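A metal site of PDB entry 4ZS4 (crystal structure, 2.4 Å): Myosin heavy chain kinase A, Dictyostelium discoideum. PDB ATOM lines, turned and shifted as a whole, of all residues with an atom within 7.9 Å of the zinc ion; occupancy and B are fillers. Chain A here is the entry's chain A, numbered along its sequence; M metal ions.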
ATOM      1  N   SER A 201     -12.268  15.042  17.487  1.00  0.00           N
ATOM      2  CA  SER A 201     -11.791  13.841  16.842  1.00  0.00           C
ATOM      3  C   SER A 201     -10.779  13.037  17.659  1.00  0.00           C
ATOM      4  O   SER A 201     -10.800  11.798  17.650  1.00  0.00           O
ATOM      5  CB  SER A 201     -11.158  14.214  15.516  1.00  0.00           C
ATOM      6  OG  SER A 201     -12.160  14.424  14.560  1.00  0.00           O
ATOM      7  N   GLN A 204     -11.885  10.237  20.203  1.00  0.00           N
ATOM      8  CA  GLN A 204     -12.544   9.085  19.624  1.00  0.00           C
ATOM      9  C   GLN A 204     -11.502   8.286  18.893  1.00  0.00           C
ATOM     10  O   GLN A 204     -11.525   7.060  18.910  1.00  0.00           O
ATOM     11  CB  GLN A 204     -13.658   9.475  18.655  1.00  0.00           C
ATOM     12  CG  GLN A 204     -14.731  10.385  19.215  1.00  0.00           C
ATOM     13  CD  GLN A 204     -15.266   9.961  20.551  1.00  0.00           C
ATOM     14  OE1 GLN A 204     -15.510   8.775  20.810  1.00  0.00           O
ATOM     15  NE2 GLN A 204     -15.524  10.947  21.418  1.00  0.00           N
ATOM     16  N   ALA A 205     -10.567   8.984  18.259  1.00  0.00           N
ATOM     17  CA  ALA A 205      -9.515   8.307  17.545  1.00  0.00           C
ATOM     18  C   ALA A 205      -8.572   7.591  18.518  1.00  0.00           C
ATOM     19  O   ALA A 205      -7.997   6.539  18.194  1.00  0.00           O
ATOM     20  CB  ALA A 205      -8.734   9.302  16.682  1.00  0.00           C
ATOM     21  N   PHE A 206      -8.392   8.160  19.721  1.00  0.00           N
ATOM     22  CA  PHE A 206      -7.542   7.518  20.689  1.00  0.00           C
ATOM     23  C   PHE A 206      -8.198   6.213  21.147  1.00  0.00           C
ATOM     24  O   PHE A 206      -7.524   5.175  21.174  1.00  0.00           O
ATOM     25  CB  PHE A 206      -7.258   8.413  21.891  1.00  0.00           C
ATOM     26  CG  PHE A 206      -6.670   7.673  23.033  1.00  0.00           C
ATOM     27  CD1 PHE A 206      -5.345   7.275  22.993  1.00  0.00           C
ATOM     28  CD2 PHE A 206      -7.441   7.327  24.112  1.00  0.00           C
ATOM     29  CE1 PHE A 206      -4.794   6.544  24.033  1.00  0.00           C
ATOM     30  CE2 PHE A 206      -6.896   6.615  25.165  1.00  0.00           C
ATOM     31  CZ  PHE A 206      -5.571   6.217  25.126  1.00  0.00           C
ATOM     32  N   SER A 207      -9.482   6.245  21.458  1.00  0.00           N
ATOM     33  CA  SER A 207     -10.216   5.032  21.815  1.00  0.00           C
ATOM     34  C   SER A 207     -10.076   3.943  20.753  1.00  0.00           C
ATOM     35  O   SER A 207      -9.723   2.797  21.059  1.00  0.00           O
ATOM     36  CB  SER A 207     -11.694   5.331  22.071  1.00  0.00           C
ATOM     37  OG  SER A 207     -11.824   6.104  23.249  1.00  0.00           O
ATOM     38  N   HIS A 208     -10.303   4.308  19.511  1.00  0.00           N
ATOM     39  CA  HIS A 208     -10.104   3.375  18.405  1.00  0.00           C
ATOM     40  C   HIS A 208      -8.653   2.867  18.271  1.00  0.00           C
ATOM     41  O   HIS A 208      -8.404   1.659  18.123  1.00  0.00           O
ATOM     42  CB  HIS A 208     -10.591   4.038  17.102  1.00  0.00           C
ATOM     43  CG  HIS A 208     -10.625   3.104  15.938  1.00  0.00           C
ATOM     44  ND1 HIS A 208     -10.855   3.538  14.645  1.00  0.00           N
ATOM     45  CD2 HIS A 208     -10.424   1.765  15.847  1.00  0.00           C
ATOM     46  CE1 HIS A 208     -10.808   2.509  13.832  1.00  0.00           C
ATOM     47  NE2 HIS A 208     -10.533   1.420  14.534  1.00  0.00           N
ATOM     48  N   PHE A 209      -7.692   3.774  18.336  1.00  0.00           N
ATOM     49  CA  PHE A 209      -6.267   3.388  18.409  1.00  0.00           C
ATOM     50  C   PHE A 209      -6.020   2.243  19.425  1.00  0.00           C
ATOM     51  O   PHE A 209      -5.383   1.220  19.082  1.00  0.00           O
ATOM     52  CB  PHE A 209      -5.438   4.583  18.810  1.00  0.00           C
ATOM     53  CG  PHE A 209      -3.953   4.322  18.870  1.00  0.00           C
ATOM     54  CD1 PHE A 209      -3.198   4.323  17.737  1.00  0.00           C
ATOM     55  CD2 PHE A 209      -3.322   4.139  20.063  1.00  0.00           C
ATOM     56  CE1 PHE A 209      -1.826   4.137  17.782  1.00  0.00           C
ATOM     57  CE2 PHE A 209      -1.962   3.941  20.122  1.00  0.00           C
ATOM     58  CZ  PHE A 209      -1.214   3.940  18.982  1.00  0.00           C
ATOM     59  N   GLU A 212      -7.395  -1.169  18.126  1.00  0.00           N
ATOM     60  CA  GLU A 212      -6.668  -1.778  17.034  1.00  0.00           C
ATOM     61  C   GLU A 212      -5.265  -2.191  17.462  1.00  0.00           C
ATOM     62  O   GLU A 212      -4.821  -3.305  17.209  1.00  0.00           O
ATOM     63  CB  GLU A 212      -6.600  -0.845  15.816  1.00  0.00           C
ATOM     64  CG  GLU A 212      -6.002  -1.564  14.604  1.00  0.00           C
ATOM     65  CD  GLU A 212      -6.229  -0.865  13.262  1.00  0.00           C
ATOM     66  OE1 GLU A 212      -7.323  -0.301  13.058  1.00  0.00           O
ATOM     67  OE2 GLU A 212      -5.305  -0.920  12.410  1.00  0.00           O
ATOM     68  N   PHE A 256     -19.002   0.696  21.892  1.00  0.00           N
ATOM     69  CA  PHE A 256     -18.121   1.673  21.293  1.00  0.00           C
ATOM     70  C   PHE A 256     -18.144   1.592  19.770  1.00  0.00           C
ATOM     71  O   PHE A 256     -18.184   2.608  19.100  1.00  0.00           O
ATOM     72  CB  PHE A 256     -16.681   1.568  21.780  1.00  0.00           C
ATOM     73  CG  PHE A 256     -15.754   2.477  21.052  1.00  0.00           C
ATOM     74  CD1 PHE A 256     -15.681   3.827  21.390  1.00  0.00           C
ATOM     75  CD2 PHE A 256     -15.019   2.013  19.974  1.00  0.00           C
ATOM     76  CE1 PHE A 256     -14.861   4.684  20.697  1.00  0.00           C
ATOM     77  CE2 PHE A 256     -14.192   2.865  19.276  1.00  0.00           C
ATOM     78  CZ  PHE A 256     -14.111   4.194  19.625  1.00  0.00           C
ATOM     79  N   HIS A 260     -19.086   4.482  16.854  1.00  0.00           N
ATOM     80  CA  HIS A 260     -17.850   5.085  16.386  1.00  0.00           C
ATOM     81  C   HIS A 260     -17.888   5.341  14.880  1.00  0.00           C
ATOM     82  O   HIS A 260     -18.147   4.431  14.111  1.00  0.00           O
ATOM     83  CB  HIS A 260     -16.606   4.222  16.692  1.00  0.00           C
ATOM     84  CG  HIS A 260     -15.336   4.832  16.167  1.00  0.00           C
ATOM     85  ND1 HIS A 260     -14.824   6.030  16.648  1.00  0.00           N
ATOM     86  CD2 HIS A 260     -14.487   4.438  15.189  1.00  0.00           C
ATOM     87  CE1 HIS A 260     -13.721   6.337  15.988  1.00  0.00           C
ATOM     88  NE2 HIS A 260     -13.498   5.393  15.088  1.00  0.00           N
ATOM     89  N   LYS A 261     -17.603   6.579  14.469  1.00  0.00           N
ATOM     90  CA  LYS A 261     -17.368   6.928  13.071  1.00  0.00           C
ATOM     91  C   LYS A 261     -15.933   7.383  12.973  1.00  0.00           C
ATOM     92  O   LYS A 261     -15.532   8.245  13.714  1.00  0.00           O
ATOM     93  CB  LYS A 261     -18.287   8.057  12.620  1.00  0.00           C
ATOM     94  CG  LYS A 261     -19.727   7.893  13.093  1.00  0.00           C
ATOM     95  CD  LYS A 261     -20.738   8.697  12.277  1.00  0.00           C
ATOM     96  CE  LYS A 261     -22.169   8.174  12.426  1.00  0.00           C
ATOM     97  NZ  LYS A 261     -22.354   6.708  12.156  1.00  0.00           N
ATOM     98  N   CYS A 262     -15.157   6.795  12.073  1.00  0.00           N
ATOM     99  CA  CYS A 262     -13.774   7.172  11.997  1.00  0.00           C
ATOM    100  C   CYS A 262     -13.694   8.614  11.514  1.00  0.00           C
ATOM    101  O   CYS A 262     -14.610   9.128  10.854  1.00  0.00           O
ATOM    102  CB  CYS A 262     -12.966   6.237  11.095  1.00  0.00           C
ATOM    103  SG  CYS A 262     -12.592   4.626  11.859  1.00  0.00           S
ATOM    104  N   ASN A 263     -12.595   9.275  11.875  1.00  0.00           N
ATOM    105  CA  ASN A 263     -12.421  10.677  11.587  1.00  0.00           C
ATOM    106  C   ASN A 263     -11.043  10.848  11.018  1.00  0.00           C
ATOM    107  O   ASN A 263     -10.339   9.864  10.796  1.00  0.00           O
ATOM    108  CB  ASN A 263     -12.635  11.492  12.865  1.00  0.00           C
ATOM    109  CG  ASN A 263     -11.661  11.106  13.989  1.00  0.00           C
ATOM    110  OD1 ASN A 263     -10.457  10.998  13.775  1.00  0.00           O
ATOM    111  ND2 ASN A 263     -12.198  10.921  15.194  1.00  0.00           N
ATOM    112  N   ALA A 264     -10.632  12.089  10.766  1.00  0.00           N
ATOM    113  CA  ALA A 264      -9.354  12.307  10.086  1.00  0.00           C
ATOM    114  C   ALA A 264      -8.164  11.743  10.871  1.00  0.00           C
ATOM    115  O   ALA A 264      -7.165  11.296  10.283  1.00  0.00           O
ATOM    116  CB  ALA A 264      -9.167  13.787   9.822  1.00  0.00           C
ATOM    117  N   VAL A 265      -8.259  11.789  12.196  1.00  0.00           N
ATOM    118  CA  VAL A 265      -7.151  11.306  13.045  1.00  0.00           C
ATOM    119  C   VAL A 265      -7.056   9.790  12.949  1.00  0.00           C
ATOM    120  O   VAL A 265      -5.977   9.265  12.774  1.00  0.00           O
ATOM    121  CB  VAL A 265      -7.287  11.717  14.521  1.00  0.00           C
ATOM    122  CG1 VAL A 265      -6.053  11.274  15.296  1.00  0.00           C
ATOM    123  CG2 VAL A 265      -7.446  13.233  14.645  1.00  0.00           C
ATOM    124  N   CYS A 266      -8.187   9.090  12.981  1.00  0.00           N
ATOM    125  CA  CYS A 266      -8.158   7.637  12.688  1.00  0.00           C
ATOM    126  C   CYS A 266      -7.482   7.407  11.341  1.00  0.00           C
ATOM    127  O   CYS A 266      -6.626   6.527  11.220  1.00  0.00           O
ATOM    128  CB  CYS A 266      -9.555   7.015  12.659  1.00  0.00           C
ATOM    129  SG  CYS A 266     -10.597   7.305  14.099  1.00  0.00           S
ATOM    130  N   ALA A 267      -7.825   8.205  10.338  1.00  0.00           N
ATOM    131  CA  ALA A 267      -7.210   8.020   9.019  1.00  0.00           C
ATOM    132  C   ALA A 267      -5.722   8.299   9.048  1.00  0.00           C
ATOM    133  O   ALA A 267      -4.933   7.602   8.453  1.00  0.00           O
ATOM    134  CB  ALA A 267      -7.890   8.895   7.975  1.00  0.00           C
ATOM    135  N   LEU A 271      -5.962   3.538  10.834  1.00  0.00           N
ATOM    136  CA  LEU A 271      -6.843   2.582  11.454  1.00  0.00           C
ATOM    137  C   LEU A 271      -7.906   2.095  10.455  1.00  0.00           C
ATOM    138  O   LEU A 271      -8.423   2.863   9.630  1.00  0.00           O
ATOM    139  CB  LEU A 271      -7.502   3.213  12.683  1.00  0.00           C
ATOM    140  CG  LEU A 271      -6.536   3.862  13.687  1.00  0.00           C
ATOM    141  CD1 LEU A 271      -7.313   4.458  14.837  1.00  0.00           C
ATOM    142  CD2 LEU A 271      -5.499   2.874  14.193  1.00  0.00           C
ATOM    143  N   ASP A 272      -8.196   0.801  10.512  1.00  0.00           N
ATOM    144  CA  ASP A 272      -9.238   0.189   9.722  1.00  0.00           C
ATOM    145  C   ASP A 272     -10.578   0.886   9.958  1.00  0.00           C
ATOM    146  O   ASP A 272     -10.906   1.193  11.075  1.00  0.00           O
ATOM    147  CB  ASP A 272      -9.350  -1.289  10.134  1.00  0.00           C
ATOM    148  CG  ASP A 272     -10.158  -2.118   9.171  1.00  0.00           C
ATOM    149  OD1 ASP A 272     -11.408  -1.976   9.165  1.00  0.00           O
ATOM    150  OD2 ASP A 272      -9.544  -2.925   8.428  1.00  0.00           O
ATOM    151  N   VAL A 273     -11.332   1.169   8.911  1.00  0.00           N
ATOM    152  CA  VAL A 273     -12.758   1.467   9.083  1.00  0.00           C
ATOM    153  C   VAL A 273     -13.559   0.156   9.055  1.00  0.00           C
ATOM    154  O   VAL A 273     -14.511  -0.024   9.811  1.00  0.00           O
ATOM    155  CB  VAL A 273     -13.280   2.433   8.019  1.00  0.00           C
ATOM    156  CG1 VAL A 273     -12.474   3.731   8.047  1.00  0.00           C
ATOM    157  CG2 VAL A 273     -13.251   1.787   6.633  1.00  0.00           C
HETATM  158 ZN    ZN M   1     -11.820   5.326  14.018  1.00  0.00          ZN
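NE2 of His 208 sits close to O of Asp 272. The backbone NH (N) of Cys 266 sits at hydrogen-bond distance from the side-chain amide oxygen (OD1) of Asn 263 (3.1 Å). The backbone carbonyl oxygen of Cys 266 lies within hydrogen-bond range of the backbone NH of Leu 271 (3.1 Å).
Of the 20 residues printed, 4 come within 4 Å of the zinc ion.
The zinc ion is bound by NE2 of His 260 (2.0 Å). A ring nitrogen (ND1) of His 208 binds the zinc ion (2.1 Å). SG of Cys 266 binds the zinc ion. The zinc ion is bound by SG of Cys 262 (2.4 Å).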
